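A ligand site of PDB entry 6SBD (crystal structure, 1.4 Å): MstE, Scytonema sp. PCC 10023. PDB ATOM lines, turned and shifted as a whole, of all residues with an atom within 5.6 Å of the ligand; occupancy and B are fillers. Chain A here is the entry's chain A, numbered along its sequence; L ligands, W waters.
The side-chain amide nitrogen of Gln 52 lies within hydrogen-bond range of the backbone carbonyl oxygen of Lys 337, at 2.8 Å. The side-chain carboxylate (OE2) of Glu 340 is in salt-bridge range of the guanidinium group (NE) of Arg 338. O of Phe 50 sits at hydrogen-bond distance from N of Ser 55 (2.8 Å). The side-chain hydroxyl (OH) of Tyr 101 sits at hydrogen-bond distance from the backbone carbonyl oxygen (O) of Ser 55, 2.8 Å away. N of Arg 312 is in hydrogen-bond range of O of Trp 211. NE1 of Trp 211 sits at hydrogen-bond distance from OG1 of Thr 149 (2.9 Å).
The side-chain amide oxygen of Gln 52 is in hydrogen-bond range of an oxygen (O3) of the ligand, at 2.6 Å. OE1 of Glu 340 is in hydrogen-bond range of O4 of the ligand (2.6 Å). The backbone NH (N) of Ala 54 is in hydrogen-bond range of an oxygen (O1) of the ligand, at 2.9 Å. N of Phe 339 sits at hydrogen-bond distance from O4 of the ligand (3.0 Å). The backbone NH of Ala 53 sits at hydrogen-bond distance from an oxygen (O1) of the ligand. O4 of the ligand sits at hydrogen-bond distance from NH1 of Arg 338 (3.2 Å).
Water W2 lies within hydrogen-bond range of an oxygen (O1) of the ligand (2.7 Å), the backbone NH (N) of Gln 52 (2.8 Å) and the backbone carbonyl oxygen (O) of Phe 50 (3.3 Å).
Merely in contact with the ligand: Phe 50 (3.5 Å), Tyr 101 (3.6 Å), Ile 313 (3.6 Å), Trp 172 (3.6 Å), Trp 211 (3.7 Å), Phe 150 (3.7 Å), Tyr 158 (3.8 Å), Leu 311 (3.9 Å), Leu 105 (3.96 Å) and Ile 159 (3.99 Å). Hydrophobic or aromatic side chains that line the ligand: Phe 50, Ala 53, Ala 54, Tyr 101, Leu 105, Phe 150, Tyr 158, Ile 159, Trp 172, Trp 211, Leu 311, Ile 313 and Phe 339. 16 residues have an atom within 4 Å of the ligand: Phe 50, Gln 52, Ala 53, Ala 54, Tyr 101, Leu 105, Phe 150, Tyr 158, Ile 159, Trp 172, Trp 211, Leu 311, Ile 313, Arg 338, Phe 339 and Glu 340.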
ATOM      1  N   PHE A  50     -10.290 -29.455  -0.653  1.00  0.00           N
ATOM      2  CA  PHE A  50     -10.309 -28.952  -2.056  1.00  0.00           C
ATOM      3  C   PHE A  50      -9.206 -27.919  -2.186  1.00  0.00           C
ATOM      4  O   PHE A  50      -9.428 -26.747  -1.901  1.00  0.00           O
ATOM      5  CB  PHE A  50     -11.690 -28.369  -2.356  1.00  0.00           C
ATOM      6  CG  PHE A  50     -12.732 -29.436  -2.492  1.00  0.00           C
ATOM      7  CD1 PHE A  50     -13.469 -29.863  -1.380  1.00  0.00           C
ATOM      8  CD2 PHE A  50     -12.933 -30.069  -3.689  1.00  0.00           C
ATOM      9  CE1 PHE A  50     -14.386 -30.889  -1.492  1.00  0.00           C
ATOM     10  CE2 PHE A  50     -13.869 -31.089  -3.809  1.00  0.00           C
ATOM     11  CZ  PHE A  50     -14.614 -31.478  -2.722  1.00  0.00           C
ATOM     12  N   PRO A  51      -7.976 -28.326  -2.524  1.00  0.00           N
ATOM     13  CA  PRO A  51      -6.821 -27.439  -2.345  1.00  0.00           C
ATOM     14  C   PRO A  51      -6.801 -26.216  -3.252  1.00  0.00           C
ATOM     15  O   PRO A  51      -6.074 -25.280  -2.961  1.00  0.00           O
ATOM     16  CB  PRO A  51      -5.631 -28.343  -2.631  1.00  0.00           C
ATOM     17  CG  PRO A  51      -6.182 -29.509  -3.354  1.00  0.00           C
ATOM     18  CD  PRO A  51      -7.609 -29.684  -2.906  1.00  0.00           C
ATOM     19  N   GLN A  52      -7.534 -26.252  -4.350  1.00  0.00           N
ATOM     20  CA  GLN A  52      -7.454 -25.093  -5.285  1.00  0.00           C
ATOM     21  C   GLN A  52      -8.111 -23.850  -4.680  1.00  0.00           C
ATOM     22  O   GLN A  52      -7.686 -22.782  -5.014  1.00  0.00           O
ATOM     23  CB  GLN A  52      -8.111 -25.473  -6.614  1.00  0.00           C
ATOM     24  CG  GLN A  52      -7.317 -26.540  -7.342  1.00  0.00           C
ATOM     25  CD  GLN A  52      -8.020 -27.135  -8.531  1.00  0.00           C
ATOM     26  OE1 GLN A  52      -9.094 -26.675  -8.901  1.00  0.00           O
ATOM     27  NE2 GLN A  52      -7.389 -28.130  -9.154  1.00  0.00           N
ATOM     28  N   ALA A  53      -9.214 -23.990  -3.923  1.00  0.00           N
ATOM     29  CA  ALA A  53      -9.967 -22.806  -3.446  1.00  0.00           C
ATOM     30  C   ALA A  53     -10.879 -23.134  -2.263  1.00  0.00           C
ATOM     31  O   ALA A  53     -10.777 -22.381  -1.293  1.00  0.00           O
ATOM     32  CB  ALA A  53     -10.725 -22.157  -4.575  1.00  0.00           C
ATOM     33  N   ALA A  54     -11.694 -24.195  -2.292  1.00  0.00           N
ATOM     34  CA  ALA A  54     -12.677 -24.390  -1.203  1.00  0.00           C
ATOM     35  C   ALA A  54     -12.085 -24.833   0.119  1.00  0.00           C
ATOM     36  O   ALA A  54     -12.756 -24.673   1.136  1.00  0.00           O
ATOM     37  CB  ALA A  54     -13.778 -25.320  -1.624  1.00  0.00           C
ATOM     38  N   SER A  55     -10.931 -25.421   0.106  1.00  0.00           N
ATOM     39  CA  SER A  55     -10.208 -25.682   1.377  1.00  0.00           C
ATOM     40  C   SER A  55     -10.909 -26.820   2.119  1.00  0.00           C
ATOM     41  O   SER A  55     -11.389 -27.800   1.500  1.00  0.00           O
ATOM     42  CB  SER A  55     -10.083 -24.352   2.125  1.00  0.00           C
ATOM     43  OG  SER A  55      -9.461 -24.418   3.329  1.00  0.00           O
ATOM     44  N   TRP A  60     -19.586 -29.218   8.358  1.00  0.00           N
ATOM     45  CA  TRP A  60     -20.118 -30.552   8.038  1.00  0.00           C
ATOM     46  C   TRP A  60     -19.404 -31.622   8.891  1.00  0.00           C
ATOM     47  O   TRP A  60     -20.070 -32.477   9.502  1.00  0.00           O
ATOM     48  CB  TRP A  60     -19.914 -30.784   6.541  1.00  0.00           C
ATOM     49  CG  TRP A  60     -20.085 -32.211   6.168  1.00  0.00           C
ATOM     50  CD1 TRP A  60     -21.056 -33.104   6.509  1.00  0.00           C
ATOM     51  CD2 TRP A  60     -19.143 -32.937   5.378  1.00  0.00           C
ATOM     52  NE1 TRP A  60     -20.807 -34.321   5.942  1.00  0.00           N
ATOM     53  CE2 TRP A  60     -19.660 -34.229   5.212  1.00  0.00           C
ATOM     54  CE3 TRP A  60     -17.979 -32.571   4.732  1.00  0.00           C
ATOM     55  CZ2 TRP A  60     -19.020 -35.176   4.425  1.00  0.00           C
ATOM     56  CZ3 TRP A  60     -17.367 -33.487   3.918  1.00  0.00           C
ATOM     57  CH2 TRP A  60     -17.861 -34.774   3.799  1.00  0.00           C
ATOM     58  N   TYR A 101     -20.398 -26.989   3.897  1.00  0.00           N
ATOM     59  CA  TYR A 101     -19.107 -27.724   4.000  1.00  0.00           C
ATOM     60  C   TYR A 101     -18.170 -26.984   4.931  1.00  0.00           C
ATOM     61  O   TYR A 101     -17.543 -27.580   5.821  1.00  0.00           O
ATOM     62  CB  TYR A 101     -18.525 -27.789   2.594  1.00  0.00           C
ATOM     63  CG  TYR A 101     -17.121 -28.366   2.476  1.00  0.00           C
ATOM     64  CD1 TYR A 101     -16.844 -29.715   2.650  1.00  0.00           C
ATOM     65  CD2 TYR A 101     -16.044 -27.526   2.181  1.00  0.00           C
ATOM     66  CE1 TYR A 101     -15.558 -30.195   2.480  1.00  0.00           C
ATOM     67  CE2 TYR A 101     -14.769 -28.025   2.024  1.00  0.00           C
ATOM     68  CZ  TYR A 101     -14.505 -29.360   2.190  1.00  0.00           C
ATOM     69  OH  TYR A 101     -13.217 -29.828   2.039  1.00  0.00           O
ATOM     70  N   LEU A 105     -18.550 -22.026   1.681  1.00  0.00           N
ATOM     71  CA  LEU A 105     -19.570 -22.707   0.861  1.00  0.00           C
ATOM     72  C   LEU A 105     -20.975 -22.260   1.245  1.00  0.00           C
ATOM     73  O   LEU A 105     -21.218 -21.782   2.352  1.00  0.00           O
ATOM     74  CB  LEU A 105     -19.408 -24.227   1.000  1.00  0.00           C
ATOM     75  CG  LEU A 105     -18.770 -24.922  -0.199  1.00  0.00           C
ATOM     76  CD1 LEU A 105     -19.638 -24.813  -1.444  1.00  0.00           C
ATOM     77  CD2 LEU A 105     -17.375 -24.362  -0.492  1.00  0.00           C
ATOM     78  N   THR A 149     -29.474 -31.968  -2.214  1.00  0.00           N
ATOM     79  CA  THR A 149     -28.373 -31.388  -1.416  1.00  0.00           C
ATOM     80  C   THR A 149     -28.352 -29.874  -1.556  1.00  0.00           C
ATOM     81  O   THR A 149     -28.249 -29.180  -0.535  1.00  0.00           O
ATOM     82  CB  THR A 149     -27.033 -31.955  -1.880  1.00  0.00           C
ATOM     83  OG1 THR A 149     -26.994 -33.386  -1.695  1.00  0.00           O
ATOM     84  CG2 THR A 149     -25.861 -31.363  -1.152  1.00  0.00           C
ATOM     85  N   PHE A 150     -28.410 -29.388  -2.793  1.00  0.00           N
ATOM     86  CA  PHE A 150     -28.144 -27.974  -3.092  1.00  0.00           C
ATOM     87  C   PHE A 150     -29.294 -27.346  -3.849  1.00  0.00           C
ATOM     88  O   PHE A 150     -29.916 -27.983  -4.699  1.00  0.00           O
ATOM     89  CB  PHE A 150     -26.951 -27.829  -4.042  1.00  0.00           C
ATOM     90  CG  PHE A 150     -25.638 -28.134  -3.402  1.00  0.00           C
ATOM     91  CD1 PHE A 150     -25.138 -27.351  -2.381  1.00  0.00           C
ATOM     92  CD2 PHE A 150     -24.869 -29.174  -3.885  1.00  0.00           C
ATOM     93  CE1 PHE A 150     -23.928 -27.649  -1.794  1.00  0.00           C
ATOM     94  CE2 PHE A 150     -23.637 -29.436  -3.324  1.00  0.00           C
ATOM     95  CZ  PHE A 150     -23.187 -28.689  -2.285  1.00  0.00           C
ATOM     96  N   ILE A 155     -25.356 -23.182  -5.616  1.00  0.00           N
ATOM     97  CA  ILE A 155     -24.112 -23.925  -5.967  1.00  0.00           C
ATOM     98  C   ILE A 155     -23.580 -23.541  -7.363  1.00  0.00           C
ATOM     99  O   ILE A 155     -22.325 -23.623  -7.565  1.00  0.00           O
ATOM    100  CB  ILE A 155     -24.343 -25.419  -5.840  1.00  0.00           C
ATOM    101  CG1 ILE A 155     -23.011 -26.198  -5.906  1.00  0.00           C
ATOM    102  CG2 ILE A 155     -25.339 -25.934  -6.877  1.00  0.00           C
ATOM    103  CD1 ILE A 155     -21.996 -25.761  -4.829  1.00  0.00           C
ATOM    104  N   TYR A 158     -20.457 -21.287  -7.601  1.00  0.00           N
ATOM    105  CA  TYR A 158     -19.094 -21.807  -7.369  1.00  0.00           C
ATOM    106  C   TYR A 158     -18.476 -22.393  -8.629  1.00  0.00           C
ATOM    107  O   TYR A 158     -17.257 -22.743  -8.565  1.00  0.00           O
ATOM    108  CB  TYR A 158     -19.126 -22.900  -6.266  1.00  0.00           C
ATOM    109  CG  TYR A 158     -19.442 -22.299  -4.903  1.00  0.00           C
ATOM    110  CD1 TYR A 158     -20.732 -21.873  -4.588  1.00  0.00           C
ATOM    111  CD2 TYR A 158     -18.429 -21.933  -4.076  1.00  0.00           C
ATOM    112  CE1 TYR A 158     -20.998 -21.239  -3.404  1.00  0.00           C
ATOM    113  CE2 TYR A 158     -18.664 -21.244  -2.900  1.00  0.00           C
ATOM    114  CZ  TYR A 158     -19.964 -20.924  -2.545  1.00  0.00           C
ATOM    115  OH  TYR A 158     -20.300 -20.201  -1.430  1.00  0.00           O
ATOM    116  N   ILE A 159     -19.236 -22.517  -9.707  1.00  0.00           N
ATOM    117  CA  ILE A 159     -18.719 -23.141 -10.973  1.00  0.00           C
ATOM    118  C   ILE A 159     -18.684 -22.066 -12.059  1.00  0.00           C
ATOM    119  O   ILE A 159     -19.778 -21.805 -12.667  1.00  0.00           O
ATOM    120  CB  ILE A 159     -19.568 -24.355 -11.421  1.00  0.00           C
ATOM    121  CG1 ILE A 159     -19.727 -25.401 -10.314  1.00  0.00           C
ATOM    122  CG2 ILE A 159     -18.995 -24.952 -12.733  1.00  0.00           C
ATOM    123  CD1 ILE A 159     -18.451 -26.003  -9.822  1.00  0.00           C
ATOM    124  N   TRP A 172     -26.467 -32.453  -9.248  1.00  0.00           N
ATOM    125  CA  TRP A 172     -26.147 -31.904  -7.926  1.00  0.00           C
ATOM    126  C   TRP A 172     -27.389 -31.367  -7.209  1.00  0.00           C
ATOM    127  O   TRP A 172     -27.314 -31.214  -5.998  1.00  0.00           O
ATOM    128  CB  TRP A 172     -25.123 -30.803  -8.066  1.00  0.00           C
ATOM    129  CG  TRP A 172     -23.750 -31.259  -8.414  1.00  0.00           C
ATOM    130  CD1 TRP A 172     -23.328 -32.543  -8.651  1.00  0.00           C
ATOM    131  CD2 TRP A 172     -22.594 -30.459  -8.544  1.00  0.00           C
ATOM    132  NE1 TRP A 172     -21.996 -32.560  -8.917  1.00  0.00           N
ATOM    133  CE2 TRP A 172     -21.521 -31.313  -8.889  1.00  0.00           C
ATOM    134  CE3 TRP A 172     -22.360 -29.100  -8.446  1.00  0.00           C
ATOM    135  CZ2 TRP A 172     -20.227 -30.865  -9.057  1.00  0.00           C
ATOM    136  CZ3 TRP A 172     -21.083 -28.635  -8.635  1.00  0.00           C
ATOM    137  CH2 TRP A 172     -20.031 -29.509  -8.926  1.00  0.00           C
ATOM    138  N   TRP A 211     -23.352 -39.044  -3.412  1.00  0.00           N
ATOM    139  CA  TRP A 211     -21.975 -38.540  -3.151  1.00  0.00           C
ATOM    140  C   TRP A 211     -21.057 -39.652  -2.628  1.00  0.00           C
ATOM    141  O   TRP A 211     -19.880 -39.621  -2.865  1.00  0.00           O
ATOM    142  CB  TRP A 211     -21.994 -37.394  -2.151  1.00  0.00           C
ATOM    143  CG  TRP A 211     -22.865 -36.245  -2.531  1.00  0.00           C
ATOM    144  CD1 TRP A 211     -24.076 -35.961  -1.998  1.00  0.00           C
ATOM    145  CD2 TRP A 211     -22.586 -35.195  -3.464  1.00  0.00           C
ATOM    146  NE1 TRP A 211     -24.605 -34.840  -2.598  1.00  0.00           N
ATOM    147  CE2 TRP A 211     -23.688 -34.341  -3.463  1.00  0.00           C
ATOM    148  CE3 TRP A 211     -21.537 -34.940  -4.347  1.00  0.00           C
ATOM    149  CZ2 TRP A 211     -23.760 -33.240  -4.327  1.00  0.00           C
ATOM    150  CZ3 TRP A 211     -21.575 -33.831  -5.150  1.00  0.00           C
ATOM    151  CH2 TRP A 211     -22.694 -32.988  -5.140  1.00  0.00           C
ATOM    152  N   LEU A 311     -15.468 -39.813  -1.051  1.00  0.00           N
ATOM    153  CA  LEU A 311     -16.479 -38.821  -1.478  1.00  0.00           C
ATOM    154  C   LEU A 311     -16.309 -38.533  -2.969  1.00  0.00           C
ATOM    155  O   LEU A 311     -15.217 -38.134  -3.385  1.00  0.00           O
ATOM    156  CB  LEU A 311     -16.258 -37.595  -0.628  1.00  0.00           C
ATOM    157  CG  LEU A 311     -17.158 -36.428  -0.903  1.00  0.00           C
ATOM    158  CD1 LEU A 311     -18.604 -36.787  -0.643  1.00  0.00           C
ATOM    159  CD2 LEU A 311     -16.750 -35.226  -0.091  1.00  0.00           C
ATOM    160  N   ARG A 312     -17.333 -38.873  -3.731  1.00  0.00           N
ATOM    161  CA  ARG A 312     -17.321 -38.651  -5.182  1.00  0.00           C
ATOM    162  C   ARG A 312     -17.672 -37.194  -5.486  1.00  0.00           C
ATOM    163  O   ARG A 312     -18.539 -36.649  -4.826  1.00  0.00           O
ATOM    164  CB  ARG A 312     -18.469 -39.444  -5.886  1.00  0.00           C
ATOM    165  CG  ARG A 312     -18.431 -40.948  -5.775  1.00  0.00           C
ATOM    166  CD  ARG A 312     -19.856 -41.400  -6.023  1.00  0.00           C
ATOM    167  NE  ARG A 312     -19.955 -42.788  -6.160  1.00  0.00           N
ATOM    168  CZ  ARG A 312     -21.083 -43.441  -6.131  1.00  0.00           C
ATOM    169  NH1 ARG A 312     -22.286 -42.873  -5.943  1.00  0.00           N
ATOM    170  NH2 ARG A 312     -20.994 -44.706  -6.307  1.00  0.00           N
ATOM    171  N   ILE A 313     -17.072 -36.649  -6.531  1.00  0.00           N
ATOM    172  CA  ILE A 313     -17.513 -35.359  -7.135  1.00  0.00           C
ATOM    173  C   ILE A 313     -18.030 -35.713  -8.519  1.00  0.00           C
ATOM    174  O   ILE A 313     -17.251 -35.725  -9.506  1.00  0.00           O
ATOM    175  CB  ILE A 313     -16.418 -34.304  -7.187  1.00  0.00           C
ATOM    176  CG1 ILE A 313     -15.906 -33.989  -5.783  1.00  0.00           C
ATOM    177  CG2 ILE A 313     -16.997 -33.042  -7.822  1.00  0.00           C
ATOM    178  CD1 ILE A 313     -14.743 -34.747  -5.406  1.00  0.00           C
ATOM    179  N   LYS A 337      -5.730 -30.148 -12.293  1.00  0.00           N
ATOM    180  CA  LYS A 337      -6.937 -30.864 -12.788  1.00  0.00           C
ATOM    181  C   LYS A 337      -8.145 -30.452 -11.957  1.00  0.00           C
ATOM    182  O   LYS A 337      -8.039 -30.302 -10.749  1.00  0.00           O
ATOM    183  CB  LYS A 337      -6.805 -32.394 -12.697  1.00  0.00           C
ATOM    184  CG  LYS A 337      -5.875 -33.035 -13.733  1.00  0.00           C
ATOM    185  CD  LYS A 337      -4.452 -32.521 -13.711  1.00  0.00           C
ATOM    186  CE  LYS A 337      -3.511 -33.306 -14.602  1.00  0.00           C
ATOM    187  NZ  LYS A 337      -2.125 -33.323 -14.071  1.00  0.00           N
ATOM    188  N   ARG A 338      -9.285 -30.317 -12.605  1.00  0.00           N
ATOM    189  CA  ARG A 338     -10.550 -30.151 -11.878  1.00  0.00           C
ATOM    190  C   ARG A 338     -10.966 -31.448 -11.181  1.00  0.00           C
ATOM    191  O   ARG A 338     -10.395 -32.526 -11.406  1.00  0.00           O
ATOM    192  CB  ARG A 338     -11.678 -29.619 -12.762  1.00  0.00           C
ATOM    193  CG  ARG A 338     -11.447 -28.183 -13.198  1.00  0.00           C
ATOM    194  CD  ARG A 338     -12.695 -27.582 -13.790  1.00  0.00           C
ATOM    195  NE  ARG A 338     -13.783 -27.562 -12.828  1.00  0.00           N
ATOM    196  CZ  ARG A 338     -14.092 -26.545 -12.022  1.00  0.00           C
ATOM    197  NH1 ARG A 338     -15.150 -26.600 -11.213  1.00  0.00           N
ATOM    198  NH2 ARG A 338     -13.369 -25.429 -12.058  1.00  0.00           N
ATOM    199  N   PHE A 339     -11.962 -31.321 -10.311  1.00  0.00           N
ATOM    200  CA  PHE A 339     -12.373 -32.390  -9.378  1.00  0.00           C
ATOM    201  C   PHE A 339     -13.564 -33.210  -9.902  1.00  0.00           C
ATOM    202  O   PHE A 339     -13.849 -34.310  -9.411  1.00  0.00           O
ATOM    203  CB  PHE A 339     -12.681 -31.770  -8.019  1.00  0.00           C
ATOM    204  CG  PHE A 339     -11.452 -31.546  -7.173  1.00  0.00           C
ATOM    205  CD1 PHE A 339     -10.591 -30.534  -7.462  1.00  0.00           C
ATOM    206  CD2 PHE A 339     -11.122 -32.455  -6.186  1.00  0.00           C
ATOM    207  CE1 PHE A 339      -9.450 -30.349  -6.695  1.00  0.00           C
ATOM    208  CE2 PHE A 339      -9.983 -32.282  -5.437  1.00  0.00           C
ATOM    209  CZ  PHE A 339      -9.126 -31.266  -5.739  1.00  0.00           C
ATOM    210  N   GLU A 340     -14.258 -32.732 -10.916  1.00  0.00           N
ATOM    211  CA  GLU A 340     -15.388 -33.499 -11.471  1.00  0.00           C
ATOM    212  C   GLU A 340     -14.859 -34.811 -12.038  1.00  0.00           C
ATOM    213  O   GLU A 340     -13.843 -34.842 -12.746  1.00  0.00           O
ATOM    214  CB  GLU A 340     -16.181 -32.740 -12.534  1.00  0.00           C
ATOM    215  CG  GLU A 340     -16.838 -31.469 -12.035  1.00  0.00           C
ATOM    216  CD  GLU A 340     -15.875 -30.317 -11.753  1.00  0.00           C
ATOM    217  OE1 GLU A 340     -16.127 -29.507 -10.804  1.00  0.00           O
ATOM    218  OE2 GLU A 340     -14.877 -30.168 -12.532  1.00  0.00           O
HETATM  219  C1  LIG L   1     -18.450 -31.436  -0.957  1.00  0.00           C
HETATM  220  C2  LIG L   1     -19.061 -31.704  -2.350  1.00  0.00           C
HETATM  221  C3  LIG L   1     -18.757 -33.126  -2.741  1.00  0.00           C
HETATM  222  C4  LIG L   1     -20.578 -31.489  -2.371  1.00  0.00           C
HETATM  223  C5  LIG L   1     -19.574 -28.435  -3.034  1.00  0.00           C
HETATM  224  C6  LIG L   1     -18.782 -30.874  -4.786  1.00  0.00           C
HETATM  225  C7  LIG L   1     -18.684 -27.979  -5.984  1.00  0.00           C
HETATM  226  C8  LIG L   1     -16.680 -27.180  -3.608  1.00  0.00           C
HETATM  227  C9  LIG L   1     -15.522 -26.997  -5.836  1.00  0.00           C
HETATM  228  C10 LIG L   1     -15.941 -28.508  -7.642  1.00  0.00           C
HETATM  229  C11 LIG L   1     -14.595 -27.926  -7.738  1.00  0.00           C
HETATM  230  C12 LIG L   1     -14.319 -27.066  -6.632  1.00  0.00           C
HETATM  231  C13 LIG L   1     -12.027 -26.763  -7.468  1.00  0.00           C
HETATM  232  C14 LIG L   1     -13.581 -28.205  -8.643  1.00  0.00           C
HETATM  233  C15 LIG L   1     -16.363 -25.776  -6.425  1.00  0.00           C
HETATM  234  C16 LIG L   1     -15.350 -26.844  -4.317  1.00  0.00           C
HETATM  235  C17 LIG L   1     -17.135 -28.610  -3.910  1.00  0.00           C
HETATM  236  C18 LIG L   1     -18.221 -29.207  -2.966  1.00  0.00           C
HETATM  237  C19 LIG L   1     -17.739 -29.093  -1.477  1.00  0.00           C
HETATM  238  C20 LIG L   1     -18.499 -30.009  -0.484  1.00  0.00           C
HETATM  239  C21 LIG L   1     -18.301 -30.745  -3.345  1.00  0.00           C
HETATM  240  C22 LIG L   1     -17.754 -30.231  -5.761  1.00  0.00           C
HETATM  241  C23 LIG L   1     -17.420 -28.759  -5.420  1.00  0.00           C
HETATM  242  C24 LIG L   1     -16.115 -28.397  -6.122  1.00  0.00           C
HETATM  243  C25 LIG L   1     -13.044 -26.511  -6.502  1.00  0.00           C
HETATM  244  C26 LIG L   1     -12.670 -25.580  -5.432  1.00  0.00           C
HETATM  245  O1  LIG L   1     -11.584 -25.760  -4.722  1.00  0.00           O
HETATM  246  O2  LIG L   1     -13.376 -24.518  -5.274  1.00  0.00           O
HETATM  247  C27 LIG L   1     -12.302 -27.639  -8.526  1.00  0.00           C
HETATM  248  O3  LIG L   1     -11.297 -27.907  -9.502  1.00  0.00           O
HETATM  249  O4  LIG L   1     -13.788 -29.051  -9.734  1.00  0.00           O
HETATM  250  O   HOH W   1     -14.823 -22.536  -3.872  1.00  0.00           O
HETATM  251  O   HOH W   2      -9.789 -27.822  -5.014  1.00  0.00           O
HETATM  252  O   HOH W   3     -13.466 -23.544  -7.632  1.00  0.00           O
